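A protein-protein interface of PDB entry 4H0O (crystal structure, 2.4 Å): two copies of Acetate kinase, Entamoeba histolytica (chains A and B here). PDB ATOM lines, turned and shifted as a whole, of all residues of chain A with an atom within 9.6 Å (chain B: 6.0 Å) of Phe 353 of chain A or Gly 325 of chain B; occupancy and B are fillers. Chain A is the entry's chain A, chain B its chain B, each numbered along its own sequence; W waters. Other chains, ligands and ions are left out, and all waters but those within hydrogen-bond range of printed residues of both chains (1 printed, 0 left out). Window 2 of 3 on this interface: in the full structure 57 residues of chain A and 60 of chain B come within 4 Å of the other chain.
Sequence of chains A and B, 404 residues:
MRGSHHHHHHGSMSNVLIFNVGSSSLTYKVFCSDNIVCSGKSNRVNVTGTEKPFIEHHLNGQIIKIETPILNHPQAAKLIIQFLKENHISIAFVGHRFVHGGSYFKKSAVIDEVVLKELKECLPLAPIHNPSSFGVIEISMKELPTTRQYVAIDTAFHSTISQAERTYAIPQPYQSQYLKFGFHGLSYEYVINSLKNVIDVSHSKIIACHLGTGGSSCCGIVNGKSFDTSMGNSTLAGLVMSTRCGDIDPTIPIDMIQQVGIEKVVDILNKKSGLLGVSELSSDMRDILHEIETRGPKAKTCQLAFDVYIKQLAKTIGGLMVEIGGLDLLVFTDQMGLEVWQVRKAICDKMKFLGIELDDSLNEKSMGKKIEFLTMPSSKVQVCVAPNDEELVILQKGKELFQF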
ATOM      1  N   ALA A 314     -15.784  13.488 -29.079  1.00  0.00           N
ATOM      2  CA  ALA A 314     -16.252  14.419 -28.057  1.00  0.00           C
ATOM      3  C   ALA A 314     -15.960  15.866 -28.451  1.00  0.00           C
ATOM      4  O   ALA A 314     -16.804  16.747 -28.279  1.00  0.00           O
ATOM      5  CB  ALA A 314     -15.611  14.094 -26.716  1.00  0.00           C
ATOM      6  N   ILE A 317     -18.454  16.862 -31.011  1.00  0.00           N
ATOM      7  CA  ILE A 317     -19.766  17.101 -30.405  1.00  0.00           C
ATOM      8  C   ILE A 317     -19.809  18.484 -29.778  1.00  0.00           C
ATOM      9  O   ILE A 317     -20.756  19.247 -29.996  1.00  0.00           O
ATOM     10  CB  ILE A 317     -20.104  16.081 -29.299  1.00  0.00           C
ATOM     11  CG1 ILE A 317     -20.038  14.649 -29.826  1.00  0.00           C
ATOM     12  CG2 ILE A 317     -21.493  16.355 -28.744  1.00  0.00           C
ATOM     13  CD1 ILE A 317     -20.942  14.405 -30.984  1.00  0.00           C
ATOM     14  N   GLY A 318     -18.781  18.793 -28.990  1.00  0.00           N
ATOM     15  CA  GLY A 318     -18.692  20.069 -28.301  1.00  0.00           C
ATOM     16  C   GLY A 318     -18.718  21.252 -29.251  1.00  0.00           C
ATOM     17  O   GLY A 318     -19.424  22.235 -29.007  1.00  0.00           O
ATOM     18  N   MET A 321     -22.203  21.636 -30.708  1.00  0.00           N
ATOM     19  CA  MET A 321     -23.147  22.112 -29.697  1.00  0.00           C
ATOM     20  C   MET A 321     -23.112  23.638 -29.568  1.00  0.00           C
ATOM     21  O   MET A 321     -24.155  24.281 -29.416  1.00  0.00           O
ATOM     22  CB  MET A 321     -22.867  21.460 -28.337  1.00  0.00           C
ATOM     23  CG  MET A 321     -23.846  21.875 -27.247  1.00  0.00           C
ATOM     24  SD  MET A 321     -23.437  21.232 -25.610  1.00  0.00           S
ATOM     25  CE  MET A 321     -21.936  22.150 -25.260  1.00  0.00           C
ATOM     26  N   VAL A 322     -21.913  24.211 -29.638  1.00  0.00           N
ATOM     27  CA  VAL A 322     -21.754  25.663 -29.557  1.00  0.00           C
ATOM     28  C   VAL A 322     -22.254  26.361 -30.827  1.00  0.00           C
ATOM     29  O   VAL A 322     -22.850  27.440 -30.759  1.00  0.00           O
ATOM     30  CB  VAL A 322     -20.298  26.057 -29.235  1.00  0.00           C
ATOM     31  CG1 VAL A 322     -20.082  27.548 -29.433  1.00  0.00           C
ATOM     32  CG2 VAL A 322     -19.962  25.678 -27.807  1.00  0.00           C
ATOM     33  N   ILE A 347     -18.497   8.416 -24.387  1.00  0.00           N
ATOM     34  CA  ILE A 347     -18.905   9.740 -24.845  1.00  0.00           C
ATOM     35  C   ILE A 347     -19.778  10.449 -23.806  1.00  0.00           C
ATOM     36  O   ILE A 347     -19.531  11.607 -23.465  1.00  0.00           O
ATOM     37  CB  ILE A 347     -19.644   9.669 -26.200  1.00  0.00           C
ATOM     38  CG1 ILE A 347     -18.686   9.226 -27.312  1.00  0.00           C
ATOM     39  CG2 ILE A 347     -20.269  11.011 -26.548  1.00  0.00           C
ATOM     40  CD1 ILE A 347     -17.411  10.041 -27.378  1.00  0.00           C
ATOM     41  N   CYS A 348     -20.791   9.753 -23.297  1.00  0.00           N
ATOM     42  CA  CYS A 348     -21.691  10.337 -22.302  1.00  0.00           C
ATOM     43  C   CYS A 348     -20.986  10.687 -20.986  1.00  0.00           C
ATOM     44  O   CYS A 348     -21.406  11.605 -20.277  1.00  0.00           O
ATOM     45  CB  CYS A 348     -22.886   9.417 -22.045  1.00  0.00           C
ATOM     46  SG  CYS A 348     -23.982   9.233 -23.478  1.00  0.00           S
ATOM     47  N   ASP A 349     -19.915   9.965 -20.667  1.00  0.00           N
ATOM     48  CA  ASP A 349     -19.134  10.272 -19.472  1.00  0.00           C
ATOM     49  C   ASP A 349     -18.435  11.620 -19.610  1.00  0.00           C
ATOM     50  O   ASP A 349     -18.372  12.398 -18.656  1.00  0.00           O
ATOM     51  CB  ASP A 349     -18.113   9.168 -19.182  1.00  0.00           C
ATOM     52  CG  ASP A 349     -18.721   7.981 -18.446  1.00  0.00           C
ATOM     53  OD1 ASP A 349     -19.863   8.101 -17.948  1.00  0.00           O
ATOM     54  OD2 ASP A 349     -18.050   6.930 -18.355  1.00  0.00           O
ATOM     55  N   LYS A 350     -17.919  11.897 -20.804  1.00  0.00           N
ATOM     56  CA  LYS A 350     -17.229  13.156 -21.067  1.00  0.00           C
ATOM     57  C   LYS A 350     -18.218  14.312 -21.173  1.00  0.00           C
ATOM     58  O   LYS A 350     -17.850  15.476 -21.005  1.00  0.00           O
ATOM     59  CB  LYS A 350     -16.383  13.059 -22.340  1.00  0.00           C
ATOM     60  CG  LYS A 350     -15.069  12.313 -22.148  1.00  0.00           C
ATOM     61  CD  LYS A 350     -14.161  12.446 -23.359  1.00  0.00           C
ATOM     62  CE  LYS A 350     -12.698  12.465 -22.937  1.00  0.00           C
ATOM     63  NZ  LYS A 350     -12.348  11.331 -22.033  1.00  0.00           N
ATOM     64  N   MET A 351     -19.478  13.987 -21.443  1.00  0.00           N
ATOM     65  CA  MET A 351     -20.520  15.001 -21.588  1.00  0.00           C
ATOM     66  C   MET A 351     -21.467  15.025 -20.390  1.00  0.00           C
ATOM     67  O   MET A 351     -22.516  15.669 -20.428  1.00  0.00           O
ATOM     68  CB  MET A 351     -21.311  14.775 -22.878  1.00  0.00           C
ATOM     69  CG  MET A 351     -20.482  14.904 -24.146  1.00  0.00           C
ATOM     70  SD  MET A 351     -21.425  14.525 -25.636  1.00  0.00           S
ATOM     71  CE  MET A 351     -22.663  15.818 -25.591  1.00  0.00           C
ATOM     72  N   LYS A 352     -21.088  14.322 -19.329  1.00  0.00           N
ATOM     73  CA  LYS A 352     -21.887  14.260 -18.106  1.00  0.00           C
ATOM     74  C   LYS A 352     -22.099  15.631 -17.453  1.00  0.00           C
ATOM     75  O   LYS A 352     -23.175  15.913 -16.922  1.00  0.00           O
ATOM     76  CB  LYS A 352     -21.253  13.275 -17.114  1.00  0.00           C
ATOM     77  CG  LYS A 352     -21.845  13.304 -15.714  1.00  0.00           C
ATOM     78  CD  LYS A 352     -21.343  12.137 -14.869  1.00  0.00           C
ATOM     79  CE  LYS A 352     -21.696  12.322 -13.398  1.00  0.00           C
ATOM     80  NZ  LYS A 352     -20.996  13.494 -12.793  1.00  0.00           N
ATOM     81  N   PHE A 353     -21.086  16.493 -17.516  1.00  0.00           N
ATOM     82  CA  PHE A 353     -21.175  17.818 -16.901  1.00  0.00           C
ATOM     83  C   PHE A 353     -22.196  18.727 -17.589  1.00  0.00           C
ATOM     84  O   PHE A 353     -22.563  19.773 -17.052  1.00  0.00           O
ATOM     85  CB  PHE A 353     -19.804  18.501 -16.872  1.00  0.00           C
ATOM     86  CG  PHE A 353     -19.338  18.985 -18.216  1.00  0.00           C
ATOM     87  CD1 PHE A 353     -18.647  18.138 -19.072  1.00  0.00           C
ATOM     88  CD2 PHE A 353     -19.582  20.291 -18.622  1.00  0.00           C
ATOM     89  CE1 PHE A 353     -18.211  18.581 -20.307  1.00  0.00           C
ATOM     90  CE2 PHE A 353     -19.150  20.739 -19.859  1.00  0.00           C
ATOM     91  CZ  PHE A 353     -18.462  19.882 -20.702  1.00  0.00           C
ATOM     92  N   LEU A 354     -22.638  18.336 -18.779  1.00  0.00           N
ATOM     93  CA  LEU A 354     -23.627  19.111 -19.518  1.00  0.00           C
ATOM     94  C   LEU A 354     -25.040  18.674 -19.144  1.00  0.00           C
ATOM     95  O   LEU A 354     -26.023  19.224 -19.647  1.00  0.00           O
ATOM     96  CB  LEU A 354     -23.407  18.963 -21.026  1.00  0.00           C
ATOM     97  CG  LEU A 354     -22.132  19.600 -21.584  1.00  0.00           C
ATOM     98  CD1 LEU A 354     -21.817  19.098 -22.988  1.00  0.00           C
ATOM     99  CD2 LEU A 354     -22.251  21.117 -21.584  1.00  0.00           C
ATOM    100  N   GLY A 355     -25.136  17.684 -18.260  1.00  0.00           N
ATOM    101  CA  GLY A 355     -26.426  17.176 -17.830  1.00  0.00           C
ATOM    102  C   GLY A 355     -26.868  15.930 -18.574  1.00  0.00           C
ATOM    103  O   GLY A 355     -27.983  15.873 -19.099  1.00  0.00           O
ATOM    104  N   ILE A 356     -25.994  14.929 -18.622  1.00  0.00           N
ATOM    105  CA  ILE A 356     -26.331  13.644 -19.227  1.00  0.00           C
ATOM    106  C   ILE A 356     -26.248  12.525 -18.194  1.00  0.00           C
ATOM    107  O   ILE A 356     -25.157  12.115 -17.788  1.00  0.00           O
ATOM    108  CB  ILE A 356     -25.424  13.312 -20.433  1.00  0.00           C
ATOM    109  CG1 ILE A 356     -25.629  14.336 -21.550  1.00  0.00           C
ATOM    110  CG2 ILE A 356     -25.708  11.908 -20.950  1.00  0.00           C
ATOM    111  CD1 ILE A 356     -24.880  14.018 -22.831  1.00  0.00           C
ATOM    112  N   GLU A 357     -27.412  12.039 -17.772  1.00  0.00           N
ATOM    113  CA  GLU A 357     -27.492  10.959 -16.799  1.00  0.00           C
ATOM    114  C   GLU A 357     -27.960   9.690 -17.507  1.00  0.00           C
ATOM    115  O   GLU A 357     -29.155   9.498 -17.743  1.00  0.00           O
ATOM    116  CB  GLU A 357     -28.457  11.334 -15.672  1.00  0.00           C
ATOM    117  CG  GLU A 357     -28.303  12.773 -15.178  1.00  0.00           C
ATOM    118  CD  GLU A 357     -26.959  13.031 -14.517  1.00  0.00           C
ATOM    119  OE1 GLU A 357     -26.662  12.368 -13.499  1.00  0.00           O
ATOM    120  OE2 GLU A 357     -26.200  13.895 -15.013  1.00  0.00           O
ATOM    121  N   SER A 379     -32.987  13.257 -17.102  1.00  0.00           N
ATOM    122  CA  SER A 379     -31.752  13.827 -17.640  1.00  0.00           C
ATOM    123  C   SER A 379     -32.014  15.053 -18.517  1.00  0.00           C
ATOM    124  O   SER A 379     -32.894  15.035 -19.379  1.00  0.00           O
ATOM    125  CB  SER A 379     -30.985  12.765 -18.432  1.00  0.00           C
ATOM    126  OG  SER A 379     -29.748  13.258 -18.902  1.00  0.00           O
ATOM    127  N   LYS A 380     -31.241  16.113 -18.288  1.00  0.00           N
ATOM    128  CA  LYS A 380     -31.377  17.363 -19.038  1.00  0.00           C
ATOM    129  C   LYS A 380     -31.198  17.149 -20.543  1.00  0.00           C
ATOM    130  O   LYS A 380     -32.000  17.628 -21.348  1.00  0.00           O
ATOM    131  CB  LYS A 380     -30.370  18.394 -18.518  1.00  0.00           C
ATOM    132  CG  LYS A 380     -30.383  19.736 -19.242  1.00  0.00           C
ATOM    133  CD  LYS A 380     -29.543  20.759 -18.479  1.00  0.00           C
ATOM    134  CE  LYS A 380     -29.587  22.139 -19.121  1.00  0.00           C
ATOM    135  NZ  LYS A 380     -28.596  22.291 -20.223  1.00  0.00           N
ATOM    136  N   VAL A 381     -30.142  16.429 -20.913  1.00  0.00           N
ATOM    137  CA  VAL A 381     -29.911  16.068 -22.306  1.00  0.00           C
ATOM    138  C   VAL A 381     -30.284  14.608 -22.502  1.00  0.00           C
ATOM    139  O   VAL A 381     -29.785  13.734 -21.787  1.00  0.00           O
ATOM    140  CB  VAL A 381     -28.437  16.263 -22.705  1.00  0.00           C
ATOM    141  CG1 VAL A 381     -28.225  15.914 -24.174  1.00  0.00           C
ATOM    142  CG2 VAL A 381     -28.007  17.686 -22.444  1.00  0.00           C
ATOM    143  N   LYS B 205     -11.258  25.128 -14.225  1.00  0.00           N
ATOM    144  CA  LYS B 205     -11.200  24.734 -15.626  1.00  0.00           C
ATOM    145  C   LYS B 205     -11.205  26.005 -16.459  1.00  0.00           C
ATOM    146  O   LYS B 205     -12.197  26.742 -16.489  1.00  0.00           O
ATOM    147  CB  LYS B 205     -12.381  23.834 -15.986  1.00  0.00           C
ATOM    148  CG  LYS B 205     -12.341  22.484 -15.292  1.00  0.00           C
ATOM    149  CD  LYS B 205     -13.612  21.689 -15.527  1.00  0.00           C
ATOM    150  CE  LYS B 205     -13.542  20.352 -14.813  1.00  0.00           C
ATOM    151  NZ  LYS B 205     -12.293  19.622 -15.162  1.00  0.00           N
ATOM    152  N   LEU B 320     -12.821  22.190 -26.699  1.00  0.00           N
ATOM    153  CA  LEU B 320     -11.892  22.157 -25.572  1.00  0.00           C
ATOM    154  C   LEU B 320     -12.620  22.013 -24.241  1.00  0.00           C
ATOM    155  O   LEU B 320     -12.118  21.365 -23.317  1.00  0.00           O
ATOM    156  CB  LEU B 320     -11.008  23.408 -25.559  1.00  0.00           C
ATOM    157  CG  LEU B 320      -9.886  23.436 -26.601  1.00  0.00           C
ATOM    158  CD1 LEU B 320      -9.146  24.762 -26.582  1.00  0.00           C
ATOM    159  CD2 LEU B 320      -8.910  22.289 -26.374  1.00  0.00           C
ATOM    160  N   MET B 321     -13.801  22.620 -24.152  1.00  0.00           N
ATOM    161  CA  MET B 321     -14.625  22.553 -22.948  1.00  0.00           C
ATOM    162  C   MET B 321     -14.995  21.111 -22.603  1.00  0.00           C
ATOM    163  O   MET B 321     -14.891  20.693 -21.445  1.00  0.00           O
ATOM    164  CB  MET B 321     -15.890  23.393 -23.132  1.00  0.00           C
ATOM    165  CG  MET B 321     -16.809  23.408 -21.925  1.00  0.00           C
ATOM    166  SD  MET B 321     -18.177  24.565 -22.147  1.00  0.00           S
ATOM    167  CE  MET B 321     -18.975  23.869 -23.596  1.00  0.00           C
ATOM    168  N   VAL B 322     -15.419  20.356 -23.613  1.00  0.00           N
ATOM    169  CA  VAL B 322     -15.781  18.956 -23.418  1.00  0.00           C
ATOM    170  C   VAL B 322     -14.557  18.126 -23.033  1.00  0.00           C
ATOM    171  O   VAL B 322     -14.646  17.224 -22.198  1.00  0.00           O
ATOM    172  CB  VAL B 322     -16.469  18.369 -24.668  1.00  0.00           C
ATOM    173  CG1 VAL B 322     -16.752  16.887 -24.485  1.00  0.00           C
ATOM    174  CG2 VAL B 322     -17.767  19.105 -24.946  1.00  0.00           C
ATOM    175  N   GLU B 323     -13.409  18.451 -23.624  1.00  0.00           N
ATOM    176  CA  GLU B 323     -12.168  17.733 -23.335  1.00  0.00           C
ATOM    177  C   GLU B 323     -11.721  17.868 -21.884  1.00  0.00           C
ATOM    178  O   GLU B 323     -11.281  16.895 -21.272  1.00  0.00           O
ATOM    179  CB  GLU B 323     -11.037  18.230 -24.230  1.00  0.00           C
ATOM    180  CG  GLU B 323     -11.082  17.737 -25.656  1.00  0.00           C
ATOM    181  CD  GLU B 323      -9.855  18.165 -26.432  1.00  0.00           C
ATOM    182  OE1 GLU B 323      -8.782  17.560 -26.223  1.00  0.00           O
ATOM    183  OE2 GLU B 323      -9.960  19.115 -27.237  1.00  0.00           O
ATOM    184  N   ILE B 324     -11.816  19.083 -21.347  1.00  0.00           N
ATOM    185  CA  ILE B 324     -11.351  19.365 -19.991  1.00  0.00           C
ATOM    186  C   ILE B 324     -12.443  19.141 -18.944  1.00  0.00           C
ATOM    187  O   ILE B 324     -12.183  19.213 -17.741  1.00  0.00           O
ATOM    188  CB  ILE B 324     -10.786  20.799 -19.862  1.00  0.00           C
ATOM    189  CG1 ILE B 324     -11.897  21.841 -20.027  1.00  0.00           C
ATOM    190  CG2 ILE B 324      -9.662  21.025 -20.874  1.00  0.00           C
ATOM    191  CD1 ILE B 324     -11.402  23.281 -19.921  1.00  0.00           C
ATOM    192  N   GLY B 325     -13.663  18.882 -19.405  1.00  0.00           N
ATOM    193  CA  GLY B 325     -14.755  18.515 -18.520  1.00  0.00           C
ATOM    194  C   GLY B 325     -15.559  19.672 -17.951  1.00  0.00           C
ATOM    195  O   GLY B 325     -16.191  19.529 -16.900  1.00  0.00           O
ATOM    196  N   GLY B 326     -15.549  20.813 -18.633  1.00  0.00           N
ATOM    197  CA  GLY B 326     -16.297  21.967 -18.161  1.00  0.00           C
ATOM    198  C   GLY B 326     -15.607  23.297 -18.405  1.00  0.00           C
ATOM    199  O   GLY B 326     -14.594  23.363 -19.104  1.00  0.00           O
ATOM    200  N   LEU B 327     -16.160  24.359 -17.825  1.00  0.00           N
ATOM    201  CA  LEU B 327     -15.654  25.711 -18.044  1.00  0.00           C
ATOM    202  C   LEU B 327     -16.059  26.657 -16.914  1.00  0.00           C
ATOM    203  O   LEU B 327     -17.247  26.924 -16.715  1.00  0.00           O
ATOM    204  CB  LEU B 327     -16.173  26.259 -19.377  1.00  0.00           C
ATOM    205  CG  LEU B 327     -15.823  27.718 -19.676  1.00  0.00           C
ATOM    206  CD1 LEU B 327     -14.320  27.874 -19.803  1.00  0.00           C
ATOM    207  CD2 LEU B 327     -16.525  28.207 -20.939  1.00  0.00           C
ATOM    208  N   LYS B 380     -22.741  32.440 -14.317  1.00  0.00           N
ATOM    209  CA  LYS B 380     -22.239  31.095 -14.042  1.00  0.00           C
ATOM    210  C   LYS B 380     -20.800  30.923 -14.526  1.00  0.00           C
ATOM    211  O   LYS B 380     -19.913  30.555 -13.749  1.00  0.00           O
ATOM    212  CB  LYS B 380     -23.141  30.047 -14.699  1.00  0.00           C
ATOM    213  CG  LYS B 380     -22.794  28.613 -14.319  1.00  0.00           C
ATOM    214  CD  LYS B 380     -23.286  27.627 -15.369  1.00  0.00           C
ATOM    215  CE  LYS B 380     -22.875  26.204 -15.025  1.00  0.00           C
ATOM    216  NZ  LYS B 380     -23.226  25.247 -16.110  1.00  0.00           N
HETATM  217  O   HOH W   1     -15.161  15.724 -20.278  1.00  0.00           O
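Met 321 of chain A touches its own counterpart, Met 321 of chain B.
Positions printed for both chains: 321, 322 and 380.
Of the 8 pairs that touch across the chains among the printed residues, 1 has its exchanged pair printed and touching as well.
The backbone NH of Gly 326 of chain B sits at hydrogen-bond distance from the backbone carbonyl oxygen of Met 321 of chain B, at 2.9 Å.
Among the printed residues, pairs that only touch across the chains: Ala 314 of chain A with Val 322 of chain B, Gly 318 of chain A with Val 322 of chain B, Met 321 of chain A with Met 321 of chain B, Lys 350 of chain A with Val 322 of chain B, Phe 353 of chain A with Met 321 of chain B, Phe 353 of chain A with Val 322 of chain B, Phe 353 of chain A with Gly 325 of chain B and Phe 353 of chain A with Gly 326 of chain B.
Of the printed residues of chain B, Ala 314 of chain A touches Val 322 (3.8 Å).
Printed residues of chain B within 4 Å of Gly 318 of chain A: Val 322.
Of the printed residues of chain B, Met 321 of chain A touches Met 321.
Met 351 of chain A touches none of the printed residues of chain B.
Ile 356 of chain A touches none of the printed residues of chain B.
Of the printed residues of chain A, Met 321 of chain B touches Met 321 and Phe 353.
Val 322 of chain B touches four residues of chain A.
No residue of chain A comes within 4 Å of Ile 324 of chain B.
Of chain A, only Phe 353 (3.5 Å) comes within 4 Å of Gly 325 of chain B.
Of chain A, only Phe 353 (3.5 Å) comes within 4 Å of Gly 326 of chain B.
Hydrophobic or aromatic side chains of chain B that line the printed part of chain A: Met 321 and Val 322.
Of the 19 printed residues of chain A, 5 touch a printed residue of chain B.
Among the printed residues, no Asp or Glu carboxylate lies within 4 Å of a Lys or Arg side-chain nitrogen of the other chain.
Water W1 lies within hydrogen-bond range of O of Val 322 of chain B (2.5 Å) and O of Lys 350 of chain A (2.8 Å).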
